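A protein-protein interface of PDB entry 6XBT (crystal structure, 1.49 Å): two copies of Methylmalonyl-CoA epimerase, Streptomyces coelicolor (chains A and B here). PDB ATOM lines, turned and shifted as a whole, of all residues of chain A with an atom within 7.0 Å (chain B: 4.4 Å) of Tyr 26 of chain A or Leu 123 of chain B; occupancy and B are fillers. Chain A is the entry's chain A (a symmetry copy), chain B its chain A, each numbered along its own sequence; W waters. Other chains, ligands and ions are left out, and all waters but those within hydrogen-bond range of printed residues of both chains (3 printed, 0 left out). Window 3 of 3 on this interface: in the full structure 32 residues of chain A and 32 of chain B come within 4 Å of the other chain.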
ATOM      1  N   GLU A  20      17.627   9.106  30.783  1.00  0.00           N
ATOM      2  CA  GLU A  20      18.519   7.960  30.532  1.00  0.00           C
ATOM      3  C   GLU A  20      19.160   8.014  29.154  1.00  0.00           C
ATOM      4  O   GLU A  20      20.336   7.718  28.993  1.00  0.00           O
ATOM      5  CB  GLU A  20      17.739   6.663  30.725  1.00  0.00           C
ATOM      6  CG  GLU A  20      18.554   5.418  30.441  1.00  0.00           C
ATOM      7  CD  GLU A  20      19.884   5.213  31.162  1.00  0.00           C
ATOM      8  OE1 GLU A  20      20.155   5.890  32.190  1.00  0.00           O
ATOM      9  OE2 GLU A  20      20.691   4.427  30.655  1.00  0.00           O
ATOM     10  N   PHE A  21      18.408   8.475  28.165  1.00  0.00           N
ATOM     11  CA  PHE A  21      18.956   8.658  26.811  1.00  0.00           C
ATOM     12  C   PHE A  21      20.136   9.632  26.816  1.00  0.00           C
ATOM     13  O   PHE A  21      21.189   9.403  26.280  1.00  0.00           O
ATOM     14  CB  PHE A  21      17.883   9.091  25.818  1.00  0.00           C
ATOM     15  CG  PHE A  21      18.466   9.581  24.523  1.00  0.00           C
ATOM     16  CD1 PHE A  21      18.947   8.712  23.552  1.00  0.00           C
ATOM     17  CD2 PHE A  21      18.605  10.938  24.320  1.00  0.00           C
ATOM     18  CE1 PHE A  21      19.552   9.195  22.410  1.00  0.00           C
ATOM     19  CE2 PHE A  21      19.233  11.406  23.186  1.00  0.00           C
ATOM     20  CZ  PHE A  21      19.694  10.537  22.248  1.00  0.00           C
ATOM     21  N   TYR A  22      19.978  10.760  27.542  1.00  0.00           N
ATOM     22  CA  TYR A  22      21.049  11.787  27.594  1.00  0.00           C
ATOM     23  C   TYR A  22      22.268  11.257  28.394  1.00  0.00           C
ATOM     24  O   TYR A  22      23.426  11.555  28.043  1.00  0.00           O
ATOM     25  CB  TYR A  22      20.537  13.154  28.120  1.00  0.00           C
ATOM     26  CG  TYR A  22      19.806  13.947  27.050  1.00  0.00           C
ATOM     27  CD1 TYR A  22      20.511  14.850  26.278  1.00  0.00           C
ATOM     28  CD2 TYR A  22      18.479  13.780  26.733  1.00  0.00           C
ATOM     29  CE1 TYR A  22      19.926  15.522  25.217  1.00  0.00           C
ATOM     30  CE2 TYR A  22      17.852  14.451  25.679  1.00  0.00           C
ATOM     31  CZ  TYR A  22      18.593  15.349  24.916  1.00  0.00           C
ATOM     32  OH  TYR A  22      18.061  15.961  23.793  1.00  0.00           O
ATOM     33  N   ARG A  23      22.012  10.494  29.452  1.00  0.00           N
ATOM     34  CA  ARG A  23      23.112   9.896  30.237  1.00  0.00           C
ATOM     35  C   ARG A  23      23.880   8.870  29.417  1.00  0.00           C
ATOM     36  O   ARG A  23      25.116   8.933  29.315  1.00  0.00           O
ATOM     37  CB  ARG A  23      22.541   9.264  31.524  1.00  0.00           C
ATOM     38  CG  ARG A  23      23.650   8.817  32.475  1.00  0.00           C
ATOM     39  CD  ARG A  23      23.256   7.655  33.376  1.00  0.00           C
ATOM     40  NE  ARG A  23      22.926   6.460  32.583  1.00  0.00           N
ATOM     41  CZ  ARG A  23      23.814   5.674  31.971  1.00  0.00           C
ATOM     42  NH1 ARG A  23      25.116   5.890  32.087  1.00  0.00           N
ATOM     43  NH2 ARG A  23      23.384   4.704  31.192  1.00  0.00           N
ATOM     44  N   ALA A  24      23.122   7.952  28.826  1.00  0.00           N
ATOM     45  CA  ALA A  24      23.721   6.822  28.080  1.00  0.00           C
ATOM     46  C   ALA A  24      24.438   7.319  26.822  1.00  0.00           C
ATOM     47  O   ALA A  24      25.560   6.862  26.515  1.00  0.00           O
ATOM     48  CB  ALA A  24      22.648   5.847  27.680  1.00  0.00           C
ATOM     49  N   THR A  25      23.881   8.315  26.150  1.00  0.00           N
ATOM     50  CA  THR A  25      24.455   8.717  24.841  1.00  0.00           C
ATOM     51  C   THR A  25      25.621   9.698  24.997  1.00  0.00           C
ATOM     52  O   THR A  25      26.622   9.647  24.261  1.00  0.00           O
ATOM     53  CB  THR A  25      23.353   9.291  23.938  1.00  0.00           C
ATOM     54  OG1 THR A  25      22.229   8.384  23.930  1.00  0.00           O
ATOM     55  CG2 THR A  25      23.844   9.534  22.530  1.00  0.00           C
ATOM     56  N   TYR A  26      25.470  10.658  25.918  1.00  0.00           N
ATOM     57  CA  TYR A  26      26.431  11.783  26.045  1.00  0.00           C
ATOM     58  C   TYR A  26      27.162  11.815  27.390  1.00  0.00           C
ATOM     59  O   TYR A  26      28.086  12.646  27.490  1.00  0.00           O
ATOM     60  CB  TYR A  26      25.682  13.101  25.888  1.00  0.00           C
ATOM     61  CG  TYR A  26      24.743  13.154  24.693  1.00  0.00           C
ATOM     62  CD1 TYR A  26      25.215  13.013  23.424  1.00  0.00           C
ATOM     63  CD2 TYR A  26      23.395  13.367  24.839  1.00  0.00           C
ATOM     64  CE1 TYR A  26      24.359  13.120  22.337  1.00  0.00           C
ATOM     65  CE2 TYR A  26      22.531  13.476  23.774  1.00  0.00           C
ATOM     66  CZ  TYR A  26      23.018  13.351  22.512  1.00  0.00           C
ATOM     67  OH  TYR A  26      22.201  13.446  21.433  1.00  0.00           O
ATOM     68  N   GLY A  27      26.732  11.030  28.331  1.00  0.00           N
ATOM     69  CA  GLY A  27      27.312  11.007  29.685  1.00  0.00           C
ATOM     70  C   GLY A  27      26.837  12.182  30.516  1.00  0.00           C
ATOM     71  O   GLY A  27      27.465  12.464  31.546  1.00  0.00           O
ATOM     72  N   PHE A  28      25.798  12.900  30.125  1.00  0.00           N
ATOM     73  CA  PHE A  28      25.271  14.015  30.926  1.00  0.00           C
ATOM     74  C   PHE A  28      24.528  13.455  32.121  1.00  0.00           C
ATOM     75  O   PHE A  28      23.607  12.642  31.989  1.00  0.00           O
ATOM     76  CB  PHE A  28      24.307  14.854  30.098  1.00  0.00           C
ATOM     77  CG  PHE A  28      24.882  15.502  28.865  1.00  0.00           C
ATOM     78  CD1 PHE A  28      26.238  15.812  28.746  1.00  0.00           C
ATOM     79  CD2 PHE A  28      24.084  15.782  27.761  1.00  0.00           C
ATOM     80  CE1 PHE A  28      26.707  16.481  27.613  1.00  0.00           C
ATOM     81  CE2 PHE A  28      24.547  16.446  26.665  1.00  0.00           C
ATOM     82  CZ  PHE A  28      25.885  16.756  26.544  1.00  0.00           C
ATOM     83  N   GLU A  29      24.803  14.012  33.291  1.00  0.00           N
ATOM     84  CA  GLU A  29      24.133  13.541  34.515  1.00  0.00           C
ATOM     85  C   GLU A  29      23.102  14.548  35.020  1.00  0.00           C
ATOM     86  O   GLU A  29      23.142  15.716  34.611  1.00  0.00           O
ATOM     87  CB  GLU A  29      25.201  13.356  35.602  1.00  0.00           C
ATOM     88  CG  GLU A  29      26.322  12.390  35.215  1.00  0.00           C
ATOM     89  CD  GLU A  29      25.982  10.912  35.290  1.00  0.00           C
ATOM     90  OE1 GLU A  29      24.866  10.552  35.722  1.00  0.00           O
ATOM     91  OE2 GLU A  29      26.835  10.100  34.871  1.00  0.00           O
ATOM     92  N   LEU A  46      20.175  19.096  33.406  1.00  0.00           N
ATOM     93  CA  LEU A  46      21.471  18.452  33.156  1.00  0.00           C
ATOM     94  C   LEU A  46      22.445  19.573  32.899  1.00  0.00           C
ATOM     95  O   LEU A  46      22.268  20.366  31.936  1.00  0.00           O
ATOM     96  CB  LEU A  46      21.389  17.544  31.924  1.00  0.00           C
ATOM     97  CG  LEU A  46      20.205  16.616  31.781  1.00  0.00           C
ATOM     98  CD1 LEU A  46      20.382  15.670  30.595  1.00  0.00           C
ATOM     99  CD2 LEU A  46      19.850  15.831  32.945  1.00  0.00           C
ATOM    100  N   LEU A  59      20.560  21.634  29.999  1.00  0.00           N
ATOM    101  CA  LEU A  59      19.375  21.098  29.292  1.00  0.00           C
ATOM    102  C   LEU A  59      18.289  20.927  30.326  1.00  0.00           C
ATOM    103  O   LEU A  59      18.574  20.301  31.387  1.00  0.00           O
ATOM    104  CB  LEU A  59      19.680  19.786  28.603  1.00  0.00           C
ATOM    105  CG  LEU A  59      20.848  19.846  27.657  1.00  0.00           C
ATOM    106  CD1 LEU A  59      21.103  18.461  27.110  1.00  0.00           C
ATOM    107  CD2 LEU A  59      20.616  20.820  26.521  1.00  0.00           C
ATOM    108  N   LEU B   2      31.390  15.548  25.187  1.00  0.00           N
ATOM    109  CA  LEU B   2      30.657  16.795  24.879  1.00  0.00           C
ATOM    110  C   LEU B   2      30.747  17.748  26.076  1.00  0.00           C
ATOM    111  O   LEU B   2      30.195  17.434  27.152  1.00  0.00           O
ATOM    112  CB  LEU B   2      29.196  16.458  24.588  1.00  0.00           C
ATOM    113  CG  LEU B   2      28.927  15.467  23.453  1.00  0.00           C
ATOM    114  CD1 LEU B   2      27.454  15.522  23.069  1.00  0.00           C
ATOM    115  CD2 LEU B   2      29.781  15.664  22.214  1.00  0.00           C
ATOM    116  N   ILE B  99      29.072   7.363  19.570  1.00  0.00           N
ATOM    117  CA  ILE B  99      27.594   7.465  19.500  1.00  0.00           C
ATOM    118  C   ILE B  99      27.096   6.501  18.405  1.00  0.00           C
ATOM    119  O   ILE B  99      26.067   5.859  18.643  1.00  0.00           O
ATOM    120  CB  ILE B  99      27.167   8.948  19.344  1.00  0.00           C
ATOM    121  CG1 ILE B  99      27.513   9.696  20.647  1.00  0.00           C
ATOM    122  CG2 ILE B  99      25.715   9.081  18.965  1.00  0.00           C
ATOM    123  CD1 ILE B  99      27.511  11.206  20.520  1.00  0.00           C
ATOM    124  N   VAL B 104      22.660   5.089  17.660  1.00  0.00           N
ATOM    125  CA  VAL B 104      22.095   6.378  17.215  1.00  0.00           C
ATOM    126  C   VAL B 104      22.624   6.682  15.814  1.00  0.00           C
ATOM    127  O   VAL B 104      23.816   6.571  15.573  1.00  0.00           O
ATOM    128  CB  VAL B 104      22.462   7.486  18.240  1.00  0.00           C
ATOM    129  CG1 VAL B 104      22.055   8.856  17.722  1.00  0.00           C
ATOM    130  CG2 VAL B 104      21.832   7.236  19.594  1.00  0.00           C
ATOM    131  N   ARG B 105      21.730   7.020  14.910  1.00  0.00           N
ATOM    132  CA  ARG B 105      22.098   7.287  13.501  1.00  0.00           C
ATOM    133  C   ARG B 105      22.950   8.567  13.423  1.00  0.00           C
ATOM    134  O   ARG B 105      22.405   9.664  13.742  1.00  0.00           O
ATOM    135  CB  ARG B 105      20.898   7.382  12.597  1.00  0.00           C
ATOM    136  CG  ARG B 105      20.333   5.985  12.255  1.00  0.00           C
ATOM    137  CD  ARG B 105      19.028   6.146  11.585  1.00  0.00           C
ATOM    138  NE  ARG B 105      17.937   6.550  12.427  1.00  0.00           N
ATOM    139  CZ  ARG B 105      16.699   6.839  12.035  1.00  0.00           C
ATOM    140  NH1 ARG B 105      16.371   6.881  10.745  1.00  0.00           N
ATOM    141  NH2 ARG B 105      15.799   7.093  12.944  1.00  0.00           N
ATOM    142  N   VAL B 106      24.173   8.433  12.989  1.00  0.00           N
ATOM    143  CA  VAL B 106      25.093   9.564  12.658  1.00  0.00           C
ATOM    144  C   VAL B 106      24.950   9.851  11.164  1.00  0.00           C
ATOM    145  O   VAL B 106      25.228   8.913  10.363  1.00  0.00           O
ATOM    146  CB  VAL B 106      26.505   9.239  13.088  1.00  0.00           C
ATOM    147  CG1 VAL B 106      27.497  10.382  12.699  1.00  0.00           C
ATOM    148  CG2 VAL B 106      26.660   8.933  14.562  1.00  0.00           C
ATOM    149  N   PHE B 122      25.859  15.353  12.524  1.00  0.00           N
ATOM    150  CA  PHE B 122      24.496  15.434  13.061  1.00  0.00           C
ATOM    151  C   PHE B 122      24.001  14.048  13.446  1.00  0.00           C
ATOM    152  O   PHE B 122      24.496  13.053  12.871  1.00  0.00           O
ATOM    153  CB  PHE B 122      23.511  16.011  12.074  1.00  0.00           C
ATOM    154  CG  PHE B 122      23.633  17.504  11.831  1.00  0.00           C
ATOM    155  CD1 PHE B 122      24.482  17.948  10.812  1.00  0.00           C
ATOM    156  CD2 PHE B 122      22.945  18.405  12.617  1.00  0.00           C
ATOM    157  CE1 PHE B 122      24.588  19.313  10.594  1.00  0.00           C
ATOM    158  CE2 PHE B 122      23.040  19.772  12.346  1.00  0.00           C
ATOM    159  CZ  PHE B 122      23.887  20.188  11.362  1.00  0.00           C
ATOM    160  N   LEU B 123      23.147  14.036  14.463  1.00  0.00           N
ATOM    161  CA  LEU B 123      22.437  12.810  14.942  1.00  0.00           C
ATOM    162  C   LEU B 123      20.990  12.912  14.546  1.00  0.00           C
ATOM    163  O   LEU B 123      20.320  13.941  14.645  1.00  0.00           O
ATOM    164  CB  LEU B 123      22.584  12.673  16.442  1.00  0.00           C
ATOM    165  CG  LEU B 123      23.970  12.804  17.002  1.00  0.00           C
ATOM    166  CD1 LEU B 123      23.955  12.644  18.504  1.00  0.00           C
ATOM    167  CD2 LEU B 123      24.961  11.830  16.366  1.00  0.00           C
ATOM    168  N   HIS B 124      20.395  11.793  14.030  1.00  0.00           N
ATOM    169  CA  HIS B 124      19.012  11.819  13.544  1.00  0.00           C
ATOM    170  C   HIS B 124      18.037  12.191  14.654  1.00  0.00           C
ATOM    171  O   HIS B 124      18.072  11.590  15.724  1.00  0.00           O
ATOM    172  CB  HIS B 124      18.693  10.432  12.972  1.00  0.00           C
ATOM    173  CG  HIS B 124      17.511  10.497  12.070  1.00  0.00           C
ATOM    174  ND1 HIS B 124      16.246  10.787  12.471  1.00  0.00           N
ATOM    175  CD2 HIS B 124      17.479  10.330  10.698  1.00  0.00           C
ATOM    176  CE1 HIS B 124      15.438  10.779  11.374  1.00  0.00           C
ATOM    177  NE2 HIS B 124      16.189  10.566  10.319  1.00  0.00           N
ATOM    178  N   PRO B 125      17.128  13.168  14.422  1.00  0.00           N
ATOM    179  CA  PRO B 125      16.188  13.606  15.452  1.00  0.00           C
ATOM    180  C   PRO B 125      15.295  12.498  15.993  1.00  0.00           C
ATOM    181  O   PRO B 125      14.874  12.514  17.135  1.00  0.00           O
ATOM    182  CB  PRO B 125      15.436  14.761  14.829  1.00  0.00           C
ATOM    183  CG  PRO B 125      15.573  14.466  13.337  1.00  0.00           C
ATOM    184  CD  PRO B 125      16.962  13.938  13.173  1.00  0.00           C
ATOM    185  N   CYS B 128      16.879  10.888  18.801  1.00  0.00           N
ATOM    186  CA  CYS B 128      17.200  11.821  19.937  1.00  0.00           C
ATOM    187  C   CYS B 128      15.949  12.454  20.513  1.00  0.00           C
ATOM    188  O   CYS B 128      15.956  13.654  20.914  1.00  0.00           O
ATOM    189  CB  CYS B 128      18.139  12.896  19.402  1.00  0.00           C
ATOM    190  SG  CYS B 128      19.719  12.318  18.765  1.00  0.00           S
ATOM    191  N   LEU B 132      17.025  17.487  16.582  1.00  0.00           N
ATOM    192  CA  LEU B 132      18.159  17.401  15.647  1.00  0.00           C
ATOM    193  C   LEU B 132      19.391  17.875  16.420  1.00  0.00           C
ATOM    194  O   LEU B 132      19.379  19.033  16.881  1.00  0.00           O
ATOM    195  CB  LEU B 132      17.883  18.200  14.369  1.00  0.00           C
ATOM    196  CG  LEU B 132      19.056  18.253  13.426  1.00  0.00           C
ATOM    197  CD1 LEU B 132      19.507  16.886  12.884  1.00  0.00           C
ATOM    198  CD2 LEU B 132      18.728  19.179  12.255  1.00  0.00           C
ATOM    199  N   THR B 133      20.404  17.053  16.504  1.00  0.00           N
ATOM    200  CA  THR B 133      21.530  17.275  17.442  1.00  0.00           C
ATOM    201  C   THR B 133      22.832  17.284  16.689  1.00  0.00           C
ATOM    202  O   THR B 133      23.172  16.317  15.989  1.00  0.00           O
ATOM    203  CB  THR B 133      21.549  16.229  18.551  1.00  0.00           C
ATOM    204  OG1 THR B 133      20.264  16.259  19.237  1.00  0.00           O
ATOM    205  CG2 THR B 133      22.657  16.475  19.556  1.00  0.00           C
ATOM    206  N   LEU B 135      27.106  17.828  16.598  1.00  0.00           N
ATOM    207  CA  LEU B 135      28.383  17.748  17.312  1.00  0.00           C
ATOM    208  C   LEU B 135      29.419  18.574  16.550  1.00  0.00           C
ATOM    209  O   LEU B 135      29.424  18.458  15.322  1.00  0.00           O
ATOM    210  CB  LEU B 135      28.864  16.297  17.468  1.00  0.00           C
ATOM    211  CG  LEU B 135      27.768  15.283  17.854  1.00  0.00           C
ATOM    212  CD1 LEU B 135      28.396  13.870  17.878  1.00  0.00           C
ATOM    213  CD2 LEU B 135      27.170  15.558  19.173  1.00  0.00           C
HETATM  214  O   HOH W   1      15.606  15.130  23.318  1.00  0.00           O
HETATM  215  O   HOH W   2      30.059  13.056  25.781  1.00  0.00           O
HETATM  216  O   HOH W   3      19.955  14.987  21.674  1.00  0.00           O
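Of the printed residues of chain A, Cys 128 of chain B touches Phe 21 and Tyr 26. Printed residues of chain A within 4 Å of Thr 133 of chain B: Tyr 26. The nearest residue of chain A that does not touch Leu 123 of chain B is Thr 25 of chain A (5.1 Å). The nearest printed residue of chain A that does not touch Cys 128 of chain B is Tyr 22 of chain A (4.2 Å).
No position is printed for both chains. Of the 7 pairs that touch across the chains among the printed residues, none has its exchanged pair printed and touching as well.
Water W1 lies within hydrogen-bond range of the side-chain hydroxyl (OH) of Tyr 22 of chain A and the backbone carbonyl oxygen (O) of Cys 128 of chain B. Water W2 bridges O of Tyr 26 of chain A (2.6 Å) and N of Leu 2 of chain B (2.9 Å). Water W3 lies within hydrogen-bond range of the side-chain hydroxyl (OH) of Tyr 26 of chain A (2.7 Å), the side-chain hydroxyl (OG1) of Thr 133 of chain B (2.8 Å) and the side-chain hydroxyl (OH) of Tyr 22 of chain A (3.0 Å).
O of Thr 133 of chain B lies within hydrogen-bond range of N of Leu 123 of chain B. The side-chain sulfur (SG) of Cys 128 of chain B is in hydrogen-bond range of the backbone carbonyl oxygen (O) of His 124 of chain B. O of Phe 21 of chain A sits at hydrogen-bond distance from OG1 of Thr 25 of chain A (2.8 Å). The backbone carbonyl oxygen of Tyr 22 of chain A sits at hydrogen-bond distance from the backbone NH of Phe 28 of chain A (3.4 Å).
Of the 13 printed residues of chain B, 5 touch a printed residue of chain A. Printed residues of chain A that touch a printed residue of chain B: Phe 21, Thr 25, Tyr 26 and Phe 28. Among the printed residues, 7 pairs touch across the chains. Among the printed residues, no Asp or Glu carboxylate lies within 4 Å of a Lys or Arg side-chain nitrogen of the other chain.
Among the printed residues, merely in contact across the chains: Phe 21 of chain A with Cys 128 of chain B (3.6 Å), Thr 25 of chain A with Ile 99 of chain B (3.7 Å), Tyr 26 of chain A with Leu 2 of chain B (3.4 Å), Tyr 26 of chain A with Leu 123 of chain B (3.5 Å), Tyr 26 of chain A with Cys 128 of chain B (3.8 Å), Tyr 26 of chain A with Thr 133 of chain B (3.6 Å) and Phe 28 of chain A with Leu 2 of chain B (3.6 Å).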
